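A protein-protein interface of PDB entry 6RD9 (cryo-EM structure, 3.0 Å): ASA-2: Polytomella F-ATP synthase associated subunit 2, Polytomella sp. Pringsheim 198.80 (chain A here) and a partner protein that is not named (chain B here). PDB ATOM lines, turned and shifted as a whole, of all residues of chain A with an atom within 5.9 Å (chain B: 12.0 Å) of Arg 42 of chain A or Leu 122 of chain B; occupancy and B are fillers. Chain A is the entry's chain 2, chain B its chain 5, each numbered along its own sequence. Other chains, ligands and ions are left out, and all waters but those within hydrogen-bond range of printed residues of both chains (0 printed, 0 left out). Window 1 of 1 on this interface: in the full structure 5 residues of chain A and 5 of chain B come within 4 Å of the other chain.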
ATOM      1  N   ASN A  40      -0.437  16.289 -14.472  1.00  0.00           N
ATOM      2  CA  ASN A  40      -0.083  15.361 -15.539  1.00  0.00           C
ATOM      3  C   ASN A  40      -1.070  15.563 -16.676  1.00  0.00           C
ATOM      4  O   ASN A  40      -2.209  15.101 -16.613  1.00  0.00           O
ATOM      5  CB  ASN A  40      -0.107  13.929 -15.033  1.00  0.00           C
ATOM      6  CG  ASN A  40       0.824  13.041 -15.791  1.00  0.00           C
ATOM      7  OD1 ASN A  40       1.600  13.501 -16.617  1.00  0.00           O
ATOM      8  ND2 ASN A  40       0.766  11.753 -15.508  1.00  0.00           N
ATOM      9  N   ARG A  41      -0.633  16.267 -17.714  1.00  0.00           N
ATOM     10  CA  ARG A  41      -1.507  16.545 -18.836  1.00  0.00           C
ATOM     11  C   ARG A  41      -1.515  15.415 -19.837  1.00  0.00           C
ATOM     12  O   ARG A  41      -2.528  15.202 -20.505  1.00  0.00           O
ATOM     13  CB  ARG A  41      -1.077  17.818 -19.541  1.00  0.00           C
ATOM     14  CG  ARG A  41      -0.954  18.998 -18.651  1.00  0.00           C
ATOM     15  CD  ARG A  41      -0.269  20.104 -19.394  1.00  0.00           C
ATOM     16  NE  ARG A  41      -0.852  20.302 -20.707  1.00  0.00           N
ATOM     17  CZ  ARG A  41      -1.882  21.098 -20.938  1.00  0.00           C
ATOM     18  NH1 ARG A  41      -2.360  21.234 -22.162  1.00  0.00           N
ATOM     19  NH2 ARG A  41      -2.432  21.766 -19.938  1.00  0.00           N
ATOM     20  N   ARG A  42      -0.400  14.698 -19.970  1.00  0.00           N
ATOM     21  CA  ARG A  42      -0.333  13.619 -20.946  1.00  0.00           C
ATOM     22  C   ARG A  42      -1.202  12.449 -20.523  1.00  0.00           C
ATOM     23  O   ARG A  42      -1.820  11.803 -21.367  1.00  0.00           O
ATOM     24  CB  ARG A  42       1.114  13.193 -21.140  1.00  0.00           C
ATOM     25  CG  ARG A  42       1.344  12.093 -22.140  1.00  0.00           C
ATOM     26  CD  ARG A  42       0.672  12.355 -23.459  1.00  0.00           C
ATOM     27  NE  ARG A  42       0.853  11.253 -24.386  1.00  0.00           N
ATOM     28  CZ  ARG A  42      -0.071  10.854 -25.242  1.00  0.00           C
ATOM     29  NH1 ARG A  42      -1.234  11.457 -25.282  1.00  0.00           N
ATOM     30  NH2 ARG A  42       0.165   9.847 -26.052  1.00  0.00           N
ATOM     31  N   LEU A  43      -1.296  12.189 -19.225  1.00  0.00           N
ATOM     32  CA  LEU A  43      -2.170  11.125 -18.753  1.00  0.00           C
ATOM     33  C   LEU A  43      -3.630  11.475 -18.951  1.00  0.00           C
ATOM     34  O   LEU A  43      -4.448  10.591 -19.203  1.00  0.00           O
ATOM     35  CB  LEU A  43      -1.886  10.837 -17.288  1.00  0.00           C
ATOM     36  CG  LEU A  43      -2.679   9.762 -16.566  1.00  0.00           C
ATOM     37  CD1 LEU A  43      -2.676   8.495 -17.358  1.00  0.00           C
ATOM     38  CD2 LEU A  43      -2.064   9.551 -15.227  1.00  0.00           C
ATOM     39  N   TRP A  44      -3.979  12.751 -18.864  1.00  0.00           N
ATOM     40  CA  TRP A  44      -5.330  13.139 -19.228  1.00  0.00           C
ATOM     41  C   TRP A  44      -5.518  13.091 -20.729  1.00  0.00           C
ATOM     42  O   TRP A  44      -6.640  12.913 -21.205  1.00  0.00           O
ATOM     43  CB  TRP A  44      -5.634  14.531 -18.715  1.00  0.00           C
ATOM     44  CG  TRP A  44      -6.415  14.576 -17.476  1.00  0.00           C
ATOM     45  CD1 TRP A  44      -5.999  15.045 -16.286  1.00  0.00           C
ATOM     46  CD2 TRP A  44      -7.765  14.157 -17.297  1.00  0.00           C
ATOM     47  NE1 TRP A  44      -6.999  14.944 -15.366  1.00  0.00           N
ATOM     48  CE2 TRP A  44      -8.098  14.400 -15.967  1.00  0.00           C
ATOM     49  CE3 TRP A  44      -8.722  13.591 -18.132  1.00  0.00           C
ATOM     50  CZ2 TRP A  44      -9.339  14.110 -15.456  1.00  0.00           C
ATOM     51  CZ3 TRP A  44      -9.951  13.298 -17.617  1.00  0.00           C
ATOM     52  CH2 TRP A  44     -10.251  13.562 -16.299  1.00  0.00           C
ATOM     53  N   GLY A  45      -4.434  13.238 -21.485  1.00  0.00           N
ATOM     54  CA  GLY A  45      -4.531  13.134 -22.922  1.00  0.00           C
ATOM     55  C   GLY A  45      -4.713  11.716 -23.404  1.00  0.00           C
ATOM     56  O   GLY A  45      -5.386  11.489 -24.405  1.00  0.00           O
ATOM     57  N   LYS A  46      -4.120  10.745 -22.713  1.00  0.00           N
ATOM     58  CA  LYS A  46      -4.314   9.356 -23.103  1.00  0.00           C
ATOM     59  C   LYS A  46      -5.722   8.885 -22.805  1.00  0.00           C
ATOM     60  O   LYS A  46      -6.200   7.942 -23.431  1.00  0.00           O
ATOM     61  CB  LYS A  46      -3.332   8.451 -22.381  1.00  0.00           C
ATOM     62  CG  LYS A  46      -1.891   8.759 -22.594  1.00  0.00           C
ATOM     63  CD  LYS A  46      -1.067   7.546 -22.302  1.00  0.00           C
ATOM     64  CE  LYS A  46       0.393   7.882 -22.187  1.00  0.00           C
ATOM     65  NZ  LYS A  46       0.725   8.399 -20.841  1.00  0.00           N
ATOM     66  N   VAL A  47      -6.386   9.499 -21.835  1.00  0.00           N
ATOM     67  CA  VAL A  47      -7.742   9.098 -21.500  1.00  0.00           C
ATOM     68  C   VAL A  47      -8.719   9.647 -22.517  1.00  0.00           C
ATOM     69  O   VAL A  47      -9.626   8.943 -22.964  1.00  0.00           O
ATOM     70  CB  VAL A  47      -8.084   9.544 -20.072  1.00  0.00           C
ATOM     71  CG1 VAL A  47      -9.515   9.273 -19.756  1.00  0.00           C
ATOM     72  CG2 VAL A  47      -7.220   8.822 -19.099  1.00  0.00           C
ATOM     73  N   LEU A  48      -8.546  10.899 -22.929  1.00  0.00           N
ATOM     74  CA  LEU A  48      -9.453  11.429 -23.930  1.00  0.00           C
ATOM     75  C   LEU A  48      -9.127  10.924 -25.321  1.00  0.00           C
ATOM     76  O   LEU A  48      -9.965  11.029 -26.212  1.00  0.00           O
ATOM     77  CB  LEU A  48      -9.448  12.951 -23.903  1.00  0.00           C
ATOM     78  CG  LEU A  48     -10.039  13.600 -22.659  1.00  0.00           C
ATOM     79  CD1 LEU A  48     -10.165  15.066 -22.866  1.00  0.00           C
ATOM     80  CD2 LEU A  48     -11.381  13.020 -22.324  1.00  0.00           C
ATOM     81  N   GLU A  49      -7.937  10.381 -25.537  1.00  0.00           N
ATOM     82  CA  GLU A  49      -7.663   9.714 -26.800  1.00  0.00           C
ATOM     83  C   GLU A  49      -8.436   8.416 -26.912  1.00  0.00           C
ATOM     84  O   GLU A  49      -8.932   8.077 -27.987  1.00  0.00           O
ATOM     85  CB  GLU A  49      -6.182   9.441 -26.934  1.00  0.00           C
ATOM     86  CG  GLU A  49      -5.446  10.538 -27.594  1.00  0.00           C
ATOM     87  CD  GLU A  49      -4.053  10.130 -27.934  1.00  0.00           C
ATOM     88  OE1 GLU A  49      -3.375   9.565 -27.057  1.00  0.00           O
ATOM     89  OE2 GLU A  49      -3.640  10.361 -29.087  1.00  0.00           O
ATOM     90  N   HIS A  76     -11.163  19.377 -24.195  1.00  0.00           N
ATOM     91  CA  HIS A  76     -10.692  19.119 -25.541  1.00  0.00           C
ATOM     92  C   HIS A  76     -11.960  19.074 -26.362  1.00  0.00           C
ATOM     93  O   HIS A  76     -12.765  18.171 -26.159  1.00  0.00           O
ATOM     94  CB  HIS A  76      -9.924  17.814 -25.633  1.00  0.00           C
ATOM     95  CG  HIS A  76      -9.401  17.524 -27.000  1.00  0.00           C
ATOM     96  ND1 HIS A  76      -9.774  16.414 -27.717  1.00  0.00           N
ATOM     97  CD2 HIS A  76      -8.551  18.214 -27.790  1.00  0.00           C
ATOM     98  CE1 HIS A  76      -9.170  16.426 -28.887  1.00  0.00           C
ATOM     99  NE2 HIS A  76      -8.425  17.511 -28.958  1.00  0.00           N
ATOM    100  N   THR A  79     -12.950  15.855 -28.579  1.00  0.00           N
ATOM    101  CA  THR A  79     -13.330  14.641 -27.878  1.00  0.00           C
ATOM    102  C   THR A  79     -14.699  14.763 -27.250  1.00  0.00           C
ATOM    103  O   THR A  79     -15.515  13.847 -27.357  1.00  0.00           O
ATOM    104  CB  THR A  79     -12.309  14.326 -26.809  1.00  0.00           C
ATOM    105  OG1 THR A  79     -11.007  14.332 -27.395  1.00  0.00           O
ATOM    106  CG2 THR A  79     -12.594  12.989 -26.227  1.00  0.00           C
ATOM    107  N   LEU B 108       4.731  -0.056 -33.380  1.00  0.00           N
ATOM    108  CA  LEU B 108       4.829   0.648 -32.082  1.00  0.00           C
ATOM    109  C   LEU B 108       6.191   0.507 -31.433  1.00  0.00           C
ATOM    110  O   LEU B 108       6.418   1.148 -30.427  1.00  0.00           O
ATOM    111  CB  LEU B 108       3.797   0.253 -31.016  1.00  0.00           C
ATOM    112  CG  LEU B 108       2.367   0.528 -31.438  1.00  0.00           C
ATOM    113  CD1 LEU B 108       1.380  -0.003 -30.417  1.00  0.00           C
ATOM    114  CD2 LEU B 108       2.202   2.010 -31.646  1.00  0.00           C
ATOM    115  N   LEU B 114       4.020   5.206 -37.921  1.00  0.00           N
ATOM    116  CA  LEU B 114       3.082   6.216 -38.354  1.00  0.00           C
ATOM    117  C   LEU B 114       2.059   6.564 -37.300  1.00  0.00           C
ATOM    118  O   LEU B 114       1.127   7.290 -37.617  1.00  0.00           O
ATOM    119  CB  LEU B 114       2.347   5.769 -39.609  1.00  0.00           C
ATOM    120  CG  LEU B 114       3.150   5.491 -40.863  1.00  0.00           C
ATOM    121  CD1 LEU B 114       2.223   5.564 -42.021  1.00  0.00           C
ATOM    122  CD2 LEU B 114       4.284   6.452 -41.050  1.00  0.00           C
ATOM    123  N   ILE B 115       2.183   6.084 -36.066  1.00  0.00           N
ATOM    124  CA  ILE B 115       1.097   6.284 -35.119  1.00  0.00           C
ATOM    125  C   ILE B 115       1.068   7.706 -34.590  1.00  0.00           C
ATOM    126  O   ILE B 115       0.015   8.188 -34.178  1.00  0.00           O
ATOM    127  CB  ILE B 115       1.186   5.236 -33.994  1.00  0.00           C
ATOM    128  CG1 ILE B 115      -0.097   5.171 -33.184  1.00  0.00           C
ATOM    129  CG2 ILE B 115       2.331   5.510 -33.084  1.00  0.00           C
ATOM    130  CD1 ILE B 115      -1.269   4.775 -33.988  1.00  0.00           C
ATOM    131  N   TRP B 116       2.172   8.428 -34.642  1.00  0.00           N
ATOM    132  CA  TRP B 116       2.167   9.813 -34.221  1.00  0.00           C
ATOM    133  C   TRP B 116       1.952  10.737 -35.385  1.00  0.00           C
ATOM    134  O   TRP B 116       1.807  11.941 -35.190  1.00  0.00           O
ATOM    135  CB  TRP B 116       3.471  10.153 -33.512  1.00  0.00           C
ATOM    136  CG  TRP B 116       3.857   9.116 -32.556  1.00  0.00           C
ATOM    137  CD1 TRP B 116       4.876   8.251 -32.678  1.00  0.00           C
ATOM    138  CD2 TRP B 116       3.208   8.805 -31.329  1.00  0.00           C
ATOM    139  NE1 TRP B 116       4.918   7.417 -31.607  1.00  0.00           N
ATOM    140  CE2 TRP B 116       3.894   7.736 -30.762  1.00  0.00           C
ATOM    141  CE3 TRP B 116       2.109   9.330 -30.656  1.00  0.00           C
ATOM    142  CZ2 TRP B 116       3.532   7.188 -29.557  1.00  0.00           C
ATOM    143  CZ3 TRP B 116       1.747   8.779 -29.467  1.00  0.00           C
ATOM    144  CH2 TRP B 116       2.452   7.722 -28.926  1.00  0.00           C
ATOM    145  N   GLN B 117       1.933  10.201 -36.590  1.00  0.00           N
ATOM    146  CA  GLN B 117       1.609  10.987 -37.751  1.00  0.00           C
ATOM    147  C   GLN B 117       0.161  10.871 -38.146  1.00  0.00           C
ATOM    148  O   GLN B 117      -0.347  11.783 -38.786  1.00  0.00           O
ATOM    149  CB  GLN B 117       2.443  10.558 -38.947  1.00  0.00           C
ATOM    150  CG  GLN B 117       3.852  10.294 -38.662  1.00  0.00           C
ATOM    151  CD  GLN B 117       4.613  10.111 -39.920  1.00  0.00           C
ATOM    152  OE1 GLN B 117       4.107  10.379 -40.991  1.00  0.00           O
ATOM    153  NE2 GLN B 117       5.832   9.639 -39.810  1.00  0.00           N
ATOM    154  N   VAL B 118      -0.509   9.775 -37.825  1.00  0.00           N
ATOM    155  CA  VAL B 118      -1.886   9.611 -38.246  1.00  0.00           C
ATOM    156  C   VAL B 118      -2.859   9.849 -37.111  1.00  0.00           C
ATOM    157  O   VAL B 118      -3.989  10.276 -37.369  1.00  0.00           O
ATOM    158  CB  VAL B 118      -2.126   8.232 -38.899  1.00  0.00           C
ATOM    159  CG1 VAL B 118      -1.132   7.993 -39.973  1.00  0.00           C
ATOM    160  CG2 VAL B 118      -2.112   7.113 -37.932  1.00  0.00           C
ATOM    161  N   LYS B 119      -2.453   9.649 -35.873  1.00  0.00           N
ATOM    162  CA  LYS B 119      -3.291   9.902 -34.713  1.00  0.00           C
ATOM    163  C   LYS B 119      -2.423  10.734 -33.796  1.00  0.00           C
ATOM    164  O   LYS B 119      -1.695  10.183 -32.963  1.00  0.00           O
ATOM    165  CB  LYS B 119      -3.726   8.611 -34.040  1.00  0.00           C
ATOM    166  CG  LYS B 119      -4.847   7.904 -34.722  1.00  0.00           C
ATOM    167  CD  LYS B 119      -6.139   8.608 -34.482  1.00  0.00           C
ATOM    168  CE  LYS B 119      -7.252   7.934 -35.225  1.00  0.00           C
ATOM    169  NZ  LYS B 119      -8.517   8.700 -35.111  1.00  0.00           N
ATOM    170  N   PRO B 120      -2.450  12.054 -33.937  1.00  0.00           N
ATOM    171  CA  PRO B 120      -1.570  12.894 -33.134  1.00  0.00           C
ATOM    172  C   PRO B 120      -1.959  12.879 -31.669  1.00  0.00           C
ATOM    173  O   PRO B 120      -3.137  12.850 -31.317  1.00  0.00           O
ATOM    174  CB  PRO B 120      -1.756  14.278 -33.751  1.00  0.00           C
ATOM    175  CG  PRO B 120      -3.011  14.225 -34.421  1.00  0.00           C
ATOM    176  CD  PRO B 120      -3.190  12.853 -34.917  1.00  0.00           C
ATOM    177  N   ALA B 121      -0.943  12.882 -30.821  1.00  0.00           N
ATOM    178  CA  ALA B 121      -1.116  12.642 -29.402  1.00  0.00           C
ATOM    179  C   ALA B 121      -1.701  13.854 -28.711  1.00  0.00           C
ATOM    180  O   ALA B 121      -1.316  14.985 -28.996  1.00  0.00           O
ATOM    181  CB  ALA B 121       0.226  12.296 -28.777  1.00  0.00           C
ATOM    182  N   LEU B 122      -2.611  13.614 -27.785  1.00  0.00           N
ATOM    183  CA  LEU B 122      -3.156  14.671 -26.955  1.00  0.00           C
ATOM    184  C   LEU B 122      -2.217  14.936 -25.796  1.00  0.00           C
ATOM    185  O   LEU B 122      -2.064  14.094 -24.915  1.00  0.00           O
ATOM    186  CB  LEU B 122      -4.523  14.274 -26.435  1.00  0.00           C
ATOM    187  CG  LEU B 122      -5.652  14.629 -27.357  1.00  0.00           C
ATOM    188  CD1 LEU B 122      -6.914  14.046 -26.853  1.00  0.00           C
ATOM    189  CD2 LEU B 122      -5.744  16.083 -27.333  1.00  0.00           C
ATOM    190  N   PHE B 123      -1.605  16.102 -25.776  1.00  0.00           N
ATOM    191  CA  PHE B 123      -0.713  16.427 -24.686  1.00  0.00           C
ATOM    192  C   PHE B 123      -1.302  17.455 -23.739  1.00  0.00           C
ATOM    193  O   PHE B 123      -1.935  18.415 -24.165  1.00  0.00           O
ATOM    194  CB  PHE B 123       0.609  16.923 -25.234  1.00  0.00           C
ATOM    195  CG  PHE B 123       1.590  15.845 -25.459  1.00  0.00           C
ATOM    196  CD1 PHE B 123       2.417  15.442 -24.445  1.00  0.00           C
ATOM    197  CD2 PHE B 123       1.682  15.221 -26.672  1.00  0.00           C
ATOM    198  CE1 PHE B 123       3.327  14.443 -24.647  1.00  0.00           C
ATOM    199  CE2 PHE B 123       2.590  14.220 -26.877  1.00  0.00           C
ATOM    200  CZ  PHE B 123       3.409  13.832 -25.863  1.00  0.00           C
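O of Phe 123 of chain B is in hydrogen-bond range of NH1 of Arg 41 of chain A.
The guanidinium group (NH1) of Arg 42 of chain A lies within hydrogen-bond range of the backbone carbonyl oxygen (O) of Leu 122 of chain B (2.8 Å).
The side-chain carboxylate (OE2) of Glu 49 of chain A lies close to the backbone carbonyl oxygen (O) of Pro 120 of chain B (3.4 Å).
The side-chain hydroxyl of Thr 79 of chain A sits at hydrogen-bond distance from a ring nitrogen (ND1) of His 76 of chain A, at 2.4 Å.
The side-chain carboxylate (OE1) of Glu 49 of chain A is in salt-bridge range of the guanidinium group (NH1) of Arg 42 of chain A, at 3.4 Å.
Trp 116 of chain B touches Arg 42 of chain A.
Arg 42 of chain A touches Ala 121 of chain B (NH2 to CB, 3.7 Å).
Arg 42 of chain A touches Phe 123 of chain B (CD to CE1, 3.6 Å).
Gly 45 of chain A touches Leu 122 of chain B (CA to O, 3.3 Å).
Ala 121 of chain B touches Glu 49 of chain A.
Glu 49 of chain A touches Leu 122 of chain B.
Leu 122 of chain B touches His 76 of chain A (CD2 to NE2, 3.4 Å).
No residue of chain B comes within 4 Å of Asn 40 of chain A.
Arg 41 of chain A touches just one residue of chain B: Phe 123 (3.5 Å).
Arg 42 of chain A touches four residues of chain B.
No residue of chain B comes within 4 Å of Lys 46 of chain A.
Of chain B, only Pro 120 (3.4 Å), Ala 121 (3.4 Å) and Leu 122 (3.7 Å) come within 4 Å of Glu 49 of chain A.
Thr 79 of chain A touches none of the printed residues of chain B.
Printed residues of chain A within 4 Å of Pro 120 of chain B: Glu 49 (3.4 Å).
Of the printed residues of chain A, Ala 121 of chain B touches Arg 42 (3.7 Å) and Glu 49 (3.4 Å).
Of the printed residues of chain A, Phe 123 of chain B touches Arg 41 and Arg 42.
Of the 11 printed residues of chain B, 5 touch a printed residue of chain A.
Printed residues of chain B that touch a printed residue of chain A: Trp 116, Pro 120, Ala 121, Leu 122 and Phe 123.
Hydrophobic or aromatic side chains of chain B that line the printed part of chain A: Trp 116, Ala 121, Leu 122 and Phe 123.
Among the printed residues, no Asp or Glu carboxylate lies within 4 Å of a Lys or Arg side-chain nitrogen of the other chain.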
